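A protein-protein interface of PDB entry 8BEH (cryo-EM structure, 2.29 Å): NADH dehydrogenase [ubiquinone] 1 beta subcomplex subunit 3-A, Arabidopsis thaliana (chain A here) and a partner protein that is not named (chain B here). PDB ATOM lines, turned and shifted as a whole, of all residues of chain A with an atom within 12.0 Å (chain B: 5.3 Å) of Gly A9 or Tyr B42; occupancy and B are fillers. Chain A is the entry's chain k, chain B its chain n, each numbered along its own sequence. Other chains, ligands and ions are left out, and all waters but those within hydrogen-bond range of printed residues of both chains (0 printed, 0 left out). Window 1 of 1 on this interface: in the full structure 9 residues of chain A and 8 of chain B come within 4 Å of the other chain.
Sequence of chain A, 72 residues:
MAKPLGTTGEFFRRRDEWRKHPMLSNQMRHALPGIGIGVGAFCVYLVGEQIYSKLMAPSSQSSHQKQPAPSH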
ATOM      1  N   PRO A   4      34.486  23.083  16.602  1.00  0.00           N
ATOM      2  CA  PRO A   4      33.531  22.662  17.566  1.00  0.00           C
ATOM      3  C   PRO A   4      34.178  23.235  18.808  1.00  0.00           C
ATOM      4  O   PRO A   4      34.046  22.673  19.850  1.00  0.00           O
ATOM      5  CB  PRO A   4      33.416  21.139  17.537  1.00  0.00           C
ATOM      6  CG  PRO A   4      34.539  20.736  16.600  1.00  0.00           C
ATOM      7  CD  PRO A   4      34.794  21.946  15.728  1.00  0.00           C
ATOM      8  N   LEU A   5      34.886  24.333  18.613  1.00  0.00           N
ATOM      9  CA  LEU A   5      35.589  24.875  19.783  1.00  0.00           C
ATOM     10  C   LEU A   5      34.567  25.428  20.806  1.00  0.00           C
ATOM     11  O   LEU A   5      34.621  25.003  21.945  1.00  0.00           O
ATOM     12  CB  LEU A   5      36.722  25.818  19.322  1.00  0.00           C
ATOM     13  CG  LEU A   5      38.137  25.268  19.449  1.00  0.00           C
ATOM     14  CD1 LEU A   5      39.164  26.392  19.475  1.00  0.00           C
ATOM     15  CD2 LEU A   5      38.275  24.401  20.693  1.00  0.00           C
ATOM     16  N   GLY A   6      33.618  26.247  20.420  1.00  0.00           N
ATOM     17  CA  GLY A   6      32.591  26.771  21.342  1.00  0.00           C
ATOM     18  C   GLY A   6      31.669  25.722  21.911  1.00  0.00           C
ATOM     19  O   GLY A   6      31.553  24.665  21.320  1.00  0.00           O
ATOM     20  N   THR A   7      31.041  26.038  23.034  1.00  0.00           N
ATOM     21  CA  THR A   7      30.132  25.077  23.653  1.00  0.00           C
ATOM     22  C   THR A   7      29.070  24.589  22.668  1.00  0.00           C
ATOM     23  O   THR A   7      28.727  23.403  22.655  1.00  0.00           O
ATOM     24  CB  THR A   7      29.505  25.684  24.916  1.00  0.00           C
ATOM     25  OG1 THR A   7      28.938  24.647  25.722  1.00  0.00           O
ATOM     26  CG2 THR A   7      28.436  26.724  24.591  1.00  0.00           C
ATOM     27  N   THR A   8      28.580  25.474  21.798  1.00  0.00           N
ATOM     28  CA  THR A   8      27.538  25.095  20.848  1.00  0.00           C
ATOM     29  C   THR A   8      28.058  24.093  19.820  1.00  0.00           C
ATOM     30  O   THR A   8      27.452  23.034  19.598  1.00  0.00           O
ATOM     31  CB  THR A   8      27.002  26.351  20.158  1.00  0.00           C
ATOM     32  OG1 THR A   8      26.643  27.317  21.150  1.00  0.00           O
ATOM     33  CG2 THR A   8      25.788  26.029  19.307  1.00  0.00           C
ATOM     34  N   GLY A   9      29.188  24.413  19.187  1.00  0.00           N
ATOM     35  CA  GLY A   9      29.768  23.497  18.222  1.00  0.00           C
ATOM     36  C   GLY A   9      30.215  22.195  18.853  1.00  0.00           C
ATOM     37  O   GLY A   9      30.128  21.135  18.236  1.00  0.00           O
ATOM     38  N   GLU A  10      30.702  22.262  20.092  1.00  0.00           N
ATOM     39  CA  GLU A  10      31.104  21.059  20.809  1.00  0.00           C
ATOM     40  C   GLU A  10      29.912  20.150  21.077  1.00  0.00           C
ATOM     41  O   GLU A  10      30.001  18.929  20.906  1.00  0.00           O
ATOM     42  CB  GLU A  10      31.794  21.455  22.115  1.00  0.00           C
ATOM     43  CG  GLU A  10      31.782  20.393  23.195  1.00  0.00           C
ATOM     44  CD  GLU A  10      32.542  19.147  22.812  1.00  0.00           C
ATOM     45  OE1 GLU A  10      33.433  19.227  21.939  1.00  0.00           O
ATOM     46  OE2 GLU A  10      32.251  18.082  23.393  1.00  0.00           O
ATOM     47  N   PHE A  11      28.784  20.731  21.487  1.00  0.00           N
ATOM     48  CA  PHE A  11      27.572  19.949  21.691  1.00  0.00           C
ATOM     49  C   PHE A  11      27.109  19.305  20.390  1.00  0.00           C
ATOM     50  O   PHE A  11      26.765  18.114  20.357  1.00  0.00           O
ATOM     51  CB  PHE A  11      26.494  20.858  22.282  1.00  0.00           C
ATOM     52  CG  PHE A  11      25.137  20.239  22.356  1.00  0.00           C
ATOM     53  CD1 PHE A  11      24.941  19.030  22.995  1.00  0.00           C
ATOM     54  CD2 PHE A  11      24.045  20.884  21.803  1.00  0.00           C
ATOM     55  CE1 PHE A  11      23.686  18.470  23.066  1.00  0.00           C
ATOM     56  CE2 PHE A  11      22.783  20.326  21.876  1.00  0.00           C
ATOM     57  CZ  PHE A  11      22.608  19.119  22.510  1.00  0.00           C
ATOM     58  N   PHE A  12      27.118  20.069  19.298  1.00  0.00           N
ATOM     59  CA  PHE A  12      26.638  19.512  18.038  1.00  0.00           C
ATOM     60  C   PHE A  12      27.590  18.454  17.485  1.00  0.00           C
ATOM     61  O   PHE A  12      27.139  17.484  16.871  1.00  0.00           O
ATOM     62  CB  PHE A  12      26.397  20.631  17.033  1.00  0.00           C
ATOM     63  CG  PHE A  12      25.110  21.364  17.264  1.00  0.00           C
ATOM     64  CD1 PHE A  12      23.910  20.676  17.312  1.00  0.00           C
ATOM     65  CD2 PHE A  12      25.101  22.735  17.458  1.00  0.00           C
ATOM     66  CE1 PHE A  12      22.720  21.343  17.537  1.00  0.00           C
ATOM     67  CE2 PHE A  12      23.912  23.407  17.684  1.00  0.00           C
ATOM     68  CZ  PHE A  12      22.723  22.712  17.723  1.00  0.00           C
ATOM     69  N   ARG A  13      28.897  18.606  17.703  1.00  0.00           N
ATOM     70  CA  ARG A  13      29.838  17.563  17.309  1.00  0.00           C
ATOM     71  C   ARG A  13      29.667  16.312  18.161  1.00  0.00           C
ATOM     72  O   ARG A  13      29.771  15.190  17.652  1.00  0.00           O
ATOM     73  CB  ARG A  13      31.271  18.076  17.406  1.00  0.00           C
ATOM     74  CG  ARG A  13      32.288  17.095  16.876  1.00  0.00           C
ATOM     75  CD  ARG A  13      33.705  17.583  17.103  1.00  0.00           C
ATOM     76  NE  ARG A  13      34.186  17.514  18.484  1.00  0.00           N
ATOM     77  CZ  ARG A  13      33.986  16.527  19.354  1.00  0.00           C
ATOM     78  NH1 ARG A  13      33.372  15.404  19.017  1.00  0.00           N
ATOM     79  NH2 ARG A  13      34.453  16.655  20.593  1.00  0.00           N
ATOM     80  N   ARG A  14      29.401  16.484  19.458  1.00  0.00           N
ATOM     81  CA  ARG A  14      29.141  15.334  20.315  1.00  0.00           C
ATOM     82  C   ARG A  14      27.919  14.560  19.844  1.00  0.00           C
ATOM     83  O   ARG A  14      27.922  13.325  19.846  1.00  0.00           O
ATOM     84  CB  ARG A  14      28.959  15.790  21.760  1.00  0.00           C
ATOM     85  CG  ARG A  14      30.238  15.826  22.553  1.00  0.00           C
ATOM     86  CD  ARG A  14      29.973  15.783  24.037  1.00  0.00           C
ATOM     87  NE  ARG A  14      30.912  16.610  24.783  1.00  0.00           N
ATOM     88  CZ  ARG A  14      30.648  17.182  25.947  1.00  0.00           C
ATOM     89  NH1 ARG A  14      29.473  17.038  26.536  1.00  0.00           N
ATOM     90  NH2 ARG A  14      31.588  17.911  26.539  1.00  0.00           N
ATOM     91  N   ARG A  15      26.860  15.268  19.444  1.00  0.00           N
ATOM     92  CA  ARG A  15      25.670  14.578  18.959  1.00  0.00           C
ATOM     93  C   ARG A  15      25.911  13.846  17.645  1.00  0.00           C
ATOM     94  O   ARG A  15      25.187  12.892  17.343  1.00  0.00           O
ATOM     95  CB  ARG A  15      24.509  15.562  18.790  1.00  0.00           C
ATOM     96  CG  ARG A  15      24.077  16.253  20.074  1.00  0.00           C
ATOM     97  CD  ARG A  15      23.493  15.289  21.085  1.00  0.00           C
ATOM     98  NE  ARG A  15      22.555  14.351  20.483  1.00  0.00           N
ATOM     99  CZ  ARG A  15      22.421  13.084  20.846  1.00  0.00           C
ATOM    100  NH1 ARG A  15      23.133  12.569  21.833  1.00  0.00           N
ATOM    101  NH2 ARG A  15      21.541  12.319  20.212  1.00  0.00           N
ATOM    102  N   ASP A  16      26.908  14.259  16.867  1.00  0.00           N
ATOM    103  CA  ASP A  16      27.171  13.685  15.555  1.00  0.00           C
ATOM    104  C   ASP A  16      28.122  12.493  15.600  1.00  0.00           C
ATOM    105  O   ASP A  16      28.658  12.113  14.556  1.00  0.00           O
ATOM    106  CB  ASP A  16      27.745  14.751  14.615  1.00  0.00           C
ATOM    107  CG  ASP A  16      26.677  15.634  13.996  1.00  0.00           C
ATOM    108  OD1 ASP A  16      25.586  15.125  13.676  1.00  0.00           O
ATOM    109  OD2 ASP A  16      26.935  16.837  13.811  1.00  0.00           O
ATOM    110  N   GLU A  17      28.337  11.897  16.775  1.00  0.00           N
ATOM    111  CA  GLU A  17      29.316  10.817  16.887  1.00  0.00           C
ATOM    112  C   GLU A  17      28.945   9.617  16.025  1.00  0.00           C
ATOM    113  O   GLU A  17      29.831   8.949  15.482  1.00  0.00           O
ATOM    114  CB  GLU A  17      29.465  10.395  18.346  1.00  0.00           C
ATOM    115  CG  GLU A  17      30.471  11.210  19.125  1.00  0.00           C
ATOM    116  CD  GLU A  17      30.228  11.157  20.621  1.00  0.00           C
ATOM    117  OE1 GLU A  17      30.271  12.220  21.274  1.00  0.00           O
ATOM    118  OE2 GLU A  17      29.992  10.048  21.144  1.00  0.00           O
ATOM    119  N   TRP A  18      27.649   9.337  15.876  1.00  0.00           N
ATOM    120  CA  TRP A  18      27.215   8.204  15.067  1.00  0.00           C
ATOM    121  C   TRP A  18      27.608   8.352  13.603  1.00  0.00           C
ATOM    122  O   TRP A  18      27.642   7.355  12.878  1.00  0.00           O
ATOM    123  CB  TRP A  18      25.701   8.025  15.189  1.00  0.00           C
ATOM    124  CG  TRP A  18      24.903   9.109  14.532  1.00  0.00           C
ATOM    125  CD1 TRP A  18      24.437  10.247  15.115  1.00  0.00           C
ATOM    126  CD2 TRP A  18      24.489   9.162  13.164  1.00  0.00           C
ATOM    127  NE1 TRP A  18      23.752  11.002  14.202  1.00  0.00           N
ATOM    128  CE2 TRP A  18      23.766  10.359  12.994  1.00  0.00           C
ATOM    129  CE3 TRP A  18      24.656   8.313  12.066  1.00  0.00           C
ATOM    130  CZ2 TRP A  18      23.211  10.729  11.776  1.00  0.00           C
ATOM    131  CZ3 TRP A  18      24.104   8.681  10.858  1.00  0.00           C
ATOM    132  CH2 TRP A  18      23.391   9.878  10.721  1.00  0.00           C
ATOM    133  N   ARG A  19      27.913   9.568  13.155  1.00  0.00           N
ATOM    134  CA  ARG A  19      28.318   9.786  11.774  1.00  0.00           C
ATOM    135  C   ARG A  19      29.702   9.228  11.471  1.00  0.00           C
ATOM    136  O   ARG A  19      30.096   9.198  10.302  1.00  0.00           O
ATOM    137  CB  ARG A  19      28.260  11.275  11.452  1.00  0.00           C
ATOM    138  CG  ARG A  19      26.854  11.755  11.151  1.00  0.00           C
ATOM    139  CD  ARG A  19      26.759  13.260  11.162  1.00  0.00           C
ATOM    140  NE  ARG A  19      25.464  13.702  11.658  1.00  0.00           N
ATOM    141  CZ  ARG A  19      24.419  13.962  10.886  1.00  0.00           C
ATOM    142  NH1 ARG A  19      24.473  13.798   9.575  1.00  0.00           N
ATOM    143  NH2 ARG A  19      23.289  14.381  11.444  1.00  0.00           N
ATOM    144  N   LYS A  20      30.443   8.791  12.486  1.00  0.00           N
ATOM    145  CA  LYS A  20      31.662   8.022  12.287  1.00  0.00           C
ATOM    146  C   LYS A  20      31.374   6.543  12.072  1.00  0.00           C
ATOM    147  O   LYS A  20      32.271   5.714  12.256  1.00  0.00           O
ATOM    148  CB  LYS A  20      32.610   8.206  13.474  1.00  0.00           C
ATOM    149  CG  LYS A  20      32.885   9.644  13.866  1.00  0.00           C
ATOM    150  CD  LYS A  20      33.091  10.537  12.656  1.00  0.00           C
ATOM    151  CE  LYS A  20      33.606  11.907  13.063  1.00  0.00           C
ATOM    152  NZ  LYS A  20      34.760  12.350  12.231  1.00  0.00           N
ATOM    153  N   HIS A  21      30.144   6.206  11.691  1.00  0.00           N
ATOM    154  CA  HIS A  21      29.783   4.830  11.386  1.00  0.00           C
ATOM    155  C   HIS A  21      30.743   4.263  10.344  1.00  0.00           C
ATOM    156  O   HIS A  21      31.071   4.952   9.370  1.00  0.00           O
ATOM    157  CB  HIS A  21      28.346   4.767  10.856  1.00  0.00           C
ATOM    158  CG  HIS A  21      27.624   3.498  11.188  1.00  0.00           C
ATOM    159  ND1 HIS A  21      27.926   2.293  10.591  1.00  0.00           N
ATOM    160  CD2 HIS A  21      26.585   3.255  12.020  1.00  0.00           C
ATOM    161  CE1 HIS A  21      27.122   1.357  11.062  1.00  0.00           C
ATOM    162  NE2 HIS A  21      26.299   1.915  11.932  1.00  0.00           N
ATOM    163  N   ARG B  38      28.425  19.247   8.342  1.00  0.00           N
ATOM    164  CA  ARG B  38      28.452  19.297   9.836  1.00  0.00           C
ATOM    165  C   ARG B  38      29.645  20.077  10.406  1.00  0.00           C
ATOM    166  O   ARG B  38      29.405  21.030  11.114  1.00  0.00           O
ATOM    167  CB  ARG B  38      28.388  17.864  10.376  1.00  0.00           C
ATOM    168  CG  ARG B  38      27.224  17.022   9.874  1.00  0.00           C
ATOM    169  CD  ARG B  38      25.826  17.588  10.037  1.00  0.00           C
ATOM    170  NE  ARG B  38      25.441  17.695  11.428  1.00  0.00           N
ATOM    171  CZ  ARG B  38      24.268  18.123  11.879  1.00  0.00           C
ATOM    172  NH1 ARG B  38      23.321  18.505  11.045  1.00  0.00           N
ATOM    173  NH2 ARG B  38      24.051  18.160  13.179  1.00  0.00           N
ATOM    174  N   HIS B  39      30.874  19.840   9.953  1.00  0.00           N
ATOM    175  CA  HIS B  39      32.054  20.429  10.582  1.00  0.00           C
ATOM    176  C   HIS B  39      32.127  21.936  10.367  1.00  0.00           C
ATOM    177  O   HIS B  39      32.612  22.658  11.245  1.00  0.00           O
ATOM    178  CB  HIS B  39      33.327  19.742  10.081  1.00  0.00           C
ATOM    179  CG  HIS B  39      33.639  20.006   8.643  1.00  0.00           C
ATOM    180  ND1 HIS B  39      34.392  21.084   8.232  1.00  0.00           N
ATOM    181  CD2 HIS B  39      33.300  19.333   7.519  1.00  0.00           C
ATOM    182  CE1 HIS B  39      34.503  21.063   6.918  1.00  0.00           C
ATOM    183  NE2 HIS B  39      33.846  20.013   6.460  1.00  0.00           N
ATOM    184  N   ILE B  40      31.626  22.397   9.215  1.00  0.00           N
ATOM    185  CA  ILE B  40      31.543  23.864   8.985  1.00  0.00           C
ATOM    186  C   ILE B  40      30.446  24.459   9.902  1.00  0.00           C
ATOM    187  O   ILE B  40      30.644  25.561  10.393  1.00  0.00           O
ATOM    188  CB  ILE B  40      31.321  24.188   7.493  1.00  0.00           C
ATOM    189  CG1 ILE B  40      32.431  23.623   6.601  1.00  0.00           C
ATOM    190  CG2 ILE B  40      31.091  25.669   7.243  1.00  0.00           C
ATOM    191  CD1 ILE B  40      32.086  23.618   5.140  1.00  0.00           C
ATOM    192  N   PHE B  41      29.342  23.726  10.108  1.00  0.00           N
ATOM    193  CA  PHE B  41      28.221  24.170  10.992  1.00  0.00           C
ATOM    194  C   PHE B  41      28.755  24.388  12.416  1.00  0.00           C
ATOM    195  O   PHE B  41      28.425  25.384  12.999  1.00  0.00           O
ATOM    196  CB  PHE B  41      26.977  23.268  10.940  1.00  0.00           C
ATOM    197  CG  PHE B  41      25.889  23.540  11.944  1.00  0.00           C
ATOM    198  CD1 PHE B  41      25.123  24.691  11.869  1.00  0.00           C
ATOM    199  CD2 PHE B  41      25.603  22.624  12.943  1.00  0.00           C
ATOM    200  CE1 PHE B  41      24.120  24.934  12.794  1.00  0.00           C
ATOM    201  CE2 PHE B  41      24.596  22.866  13.861  1.00  0.00           C
ATOM    202  CZ  PHE B  41      23.851  24.016  13.780  1.00  0.00           C
ATOM    203  N   TYR B  42      29.615  23.501  12.880  1.00  0.00           N
ATOM    204  CA  TYR B  42      30.094  23.643  14.256  1.00  0.00           C
ATOM    205  C   TYR B  42      30.678  25.033  14.496  1.00  0.00           C
ATOM    206  O   TYR B  42      30.270  25.748  15.426  1.00  0.00           O
ATOM    207  CB  TYR B  42      31.141  22.570  14.575  1.00  0.00           C
ATOM    208  CG  TYR B  42      30.711  21.144  14.321  1.00  0.00           C
ATOM    209  CD1 TYR B  42      29.379  20.766  14.422  1.00  0.00           C
ATOM    210  CD2 TYR B  42      31.648  20.166  13.999  1.00  0.00           C
ATOM    211  CE1 TYR B  42      28.987  19.464  14.192  1.00  0.00           C
ATOM    212  CE2 TYR B  42      31.268  18.864  13.771  1.00  0.00           C
ATOM    213  CZ  TYR B  42      29.937  18.517  13.869  1.00  0.00           C
ATOM    214  OH  TYR B  42      29.556  17.221  13.644  1.00  0.00           O
ATOM    215  N   ARG B  43      31.669  25.416  13.686  1.00  0.00           N
ATOM    216  CA  ARG B  43      32.246  26.763  13.786  1.00  0.00           C
ATOM    217  C   ARG B  43      31.211  27.890  13.549  1.00  0.00           C
ATOM    218  O   ARG B  43      31.224  28.857  14.276  1.00  0.00           O
ATOM    219  CB  ARG B  43      33.399  26.825  12.784  1.00  0.00           C
ATOM    220  CG  ARG B  43      34.223  28.101  12.850  1.00  0.00           C
ATOM    221  CD  ARG B  43      34.618  28.544  14.247  1.00  0.00           C
ATOM    222  NE  ARG B  43      35.194  27.499  15.080  1.00  0.00           N
ATOM    223  CZ  ARG B  43      36.486  27.202  15.142  1.00  0.00           C
ATOM    224  NH1 ARG B  43      37.359  27.871  14.411  1.00  0.00           N
ATOM    225  NH2 ARG B  43      36.901  26.232  15.937  1.00  0.00           N
ATOM    226  N   ASP B  44      30.374  27.748  12.560  1.00  0.00           N
ATOM    227  CA  ASP B  44      29.421  28.820  12.281  1.00  0.00           C
ATOM    228  C   ASP B  44      28.450  29.017  13.442  1.00  0.00           C
ATOM    229  O   ASP B  44      28.146  30.156  13.828  1.00  0.00           O
ATOM    230  CB  ASP B  44      28.685  28.520  10.981  1.00  0.00           C
ATOM    231  CG  ASP B  44      29.420  29.043   9.766  1.00  0.00           C
ATOM    232  OD1 ASP B  44      29.160  30.195   9.365  1.00  0.00           O
ATOM    233  OD2 ASP B  44      30.267  28.309   9.217  1.00  0.00           O
ATOM    234  N   ALA B  45      27.971  27.916  14.025  1.00  0.00           N
ATOM    235  CA  ALA B  45      27.094  27.986  15.184  1.00  0.00           C
ATOM    236  C   ALA B  45      27.802  28.603  16.380  1.00  0.00           C
ATOM    237  O   ALA B  45      27.212  29.410  17.107  1.00  0.00           O
ATOM    238  CB  ALA B  45      26.574  26.588  15.522  1.00  0.00           C
ATOM    239  N   SER B  46      29.046  28.179  16.631  1.00  0.00           N
ATOM    240  CA  SER B  46      29.864  28.809  17.713  1.00  0.00           C
ATOM    241  C   SER B  46      29.970  30.326  17.523  1.00  0.00           C
ATOM    242  O   SER B  46      29.705  31.021  18.487  1.00  0.00           O
ATOM    243  CB  SER B  46      31.197  28.229  17.826  1.00  0.00           C
ATOM    244  OG  SER B  46      31.157  26.940  18.408  1.00  0.00           O
ATOM    245  N   ASP B  47      30.222  30.801  16.302  1.00  0.00           N
ATOM    246  CA  ASP B  47      30.351  32.235  16.049  1.00  0.00           C
ATOM    247  C   ASP B  47      29.027  32.968  16.260  1.00  0.00           C
ATOM    248  O   ASP B  47      28.997  34.070  16.828  1.00  0.00           O
ATOM    249  CB  ASP B  47      30.876  32.466  14.633  1.00  0.00           C
ATOM    250  CG  ASP B  47      32.333  32.072  14.479  1.00  0.00           C
ATOM    251  OD1 ASP B  47      33.017  31.893  15.508  1.00  0.00           O
ATOM    252  OD2 ASP B  47      32.796  31.944  13.325  1.00  0.00           O
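OD2 of Asp A16 lies within salt-bridge range of NE of Arg B38 (2.9 Å). The side-chain carboxylate of Asp A16 lies within hydrogen-bond range of the side-chain hydroxyl of Tyr B42, 2.7 Å away. The backbone NH (N) of Gly A9 lies within hydrogen-bond range of the side-chain hydroxyl (OG) of Ser B46. The side-chain hydroxyl of Ser B46 sits at hydrogen-bond distance from the backbone NH of Gly A6.
NH2 of Arg A13 lies within salt-bridge range of OE1 of Glu A10 (3.1 Å). The backbone carbonyl oxygen (O) of Tyr B42 is in hydrogen-bond range of the side-chain hydroxyl (OG) of Ser B46 (3.3 Å). OD1 of Asp A16 lies within salt-bridge range of NE of Arg A19, 2.5 Å away. N of Glu A10 sits at hydrogen-bond distance from O of Pro A4, 3.4 Å away.
Pro A4 touches Tyr B42 (CA to CB, 3.8 Å). Arg B43 touches Leu A5. Thr A8 touches Ala B45. O of Tyr B42 touches CA of Gly A9 (3.6 Å). CD2 of Phe A12 touches CE2 of Phe B41 (3.6 Å). Phe A12 touches Tyr B42. Arg A13 touches Tyr B42 (CA to CZ, 3.6 Å). Arg A19 touches Arg B38.
Gly A9 touches just these residues of chain B: Tyr B42 (3.6 Å) and Ser B46 (3.3 Å). Tyr B42 touches just these residues of chain A: Pro A4, Gly A9, Phe A12, Arg A13 and Asp A16. Of chain A, only Asp A16 and Arg A19 come within 4 Å of Arg B38. His B39 touches none of the printed residues of chain A. Of chain A, only Leu A5 (3.4 Å) comes within 4 Å of Arg B43. No residue of chain A comes within 4 Å of Asp B44. Ser B46 touches just these residues of chain A: Gly A6 (3.3 Å) and Gly A9 (3.3 Å). Printed residues of chain B within 4 Å of Pro A4: Tyr B42 (3.8 Å). Printed residues of chain B within 4 Å of Phe A12: Phe B41 (3.6 Å) and Tyr B42 (3.7 Å). Glu A17 touches none of the printed residues of chain B. The nearest residue of chain B that does not touch Gly A9 is Ala B45 (5.0 Å). The nearest residue of chain A that does not touch Tyr B42 is Thr A8 (5.2 Å). The nearest printed residue of chain B that does not touch Arg A13 is Arg B38 (6.6 Å).
Printed residues of chain A that touch a printed residue of chain B: Pro A4, Leu A5, Gly A6, Thr A8, Gly A9, Phe A12, Arg A13, Asp A16 and Arg A19. Hydrophobic or aromatic side chains of chain A within 4 Å of the printed part of chain B: Pro A4, Leu A5 and Phe A12. Printed residues of chain B that touch a printed residue of chain A: Arg B38, Phe B41, Tyr B42, Arg B43, Ala B45 and Ser B46. Hydrophobic or aromatic side chains of chain B that line the printed part of chain A: Phe B41, Tyr B42 and Ala B45. Among the printed residues, 12 pairs touch across the chains.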
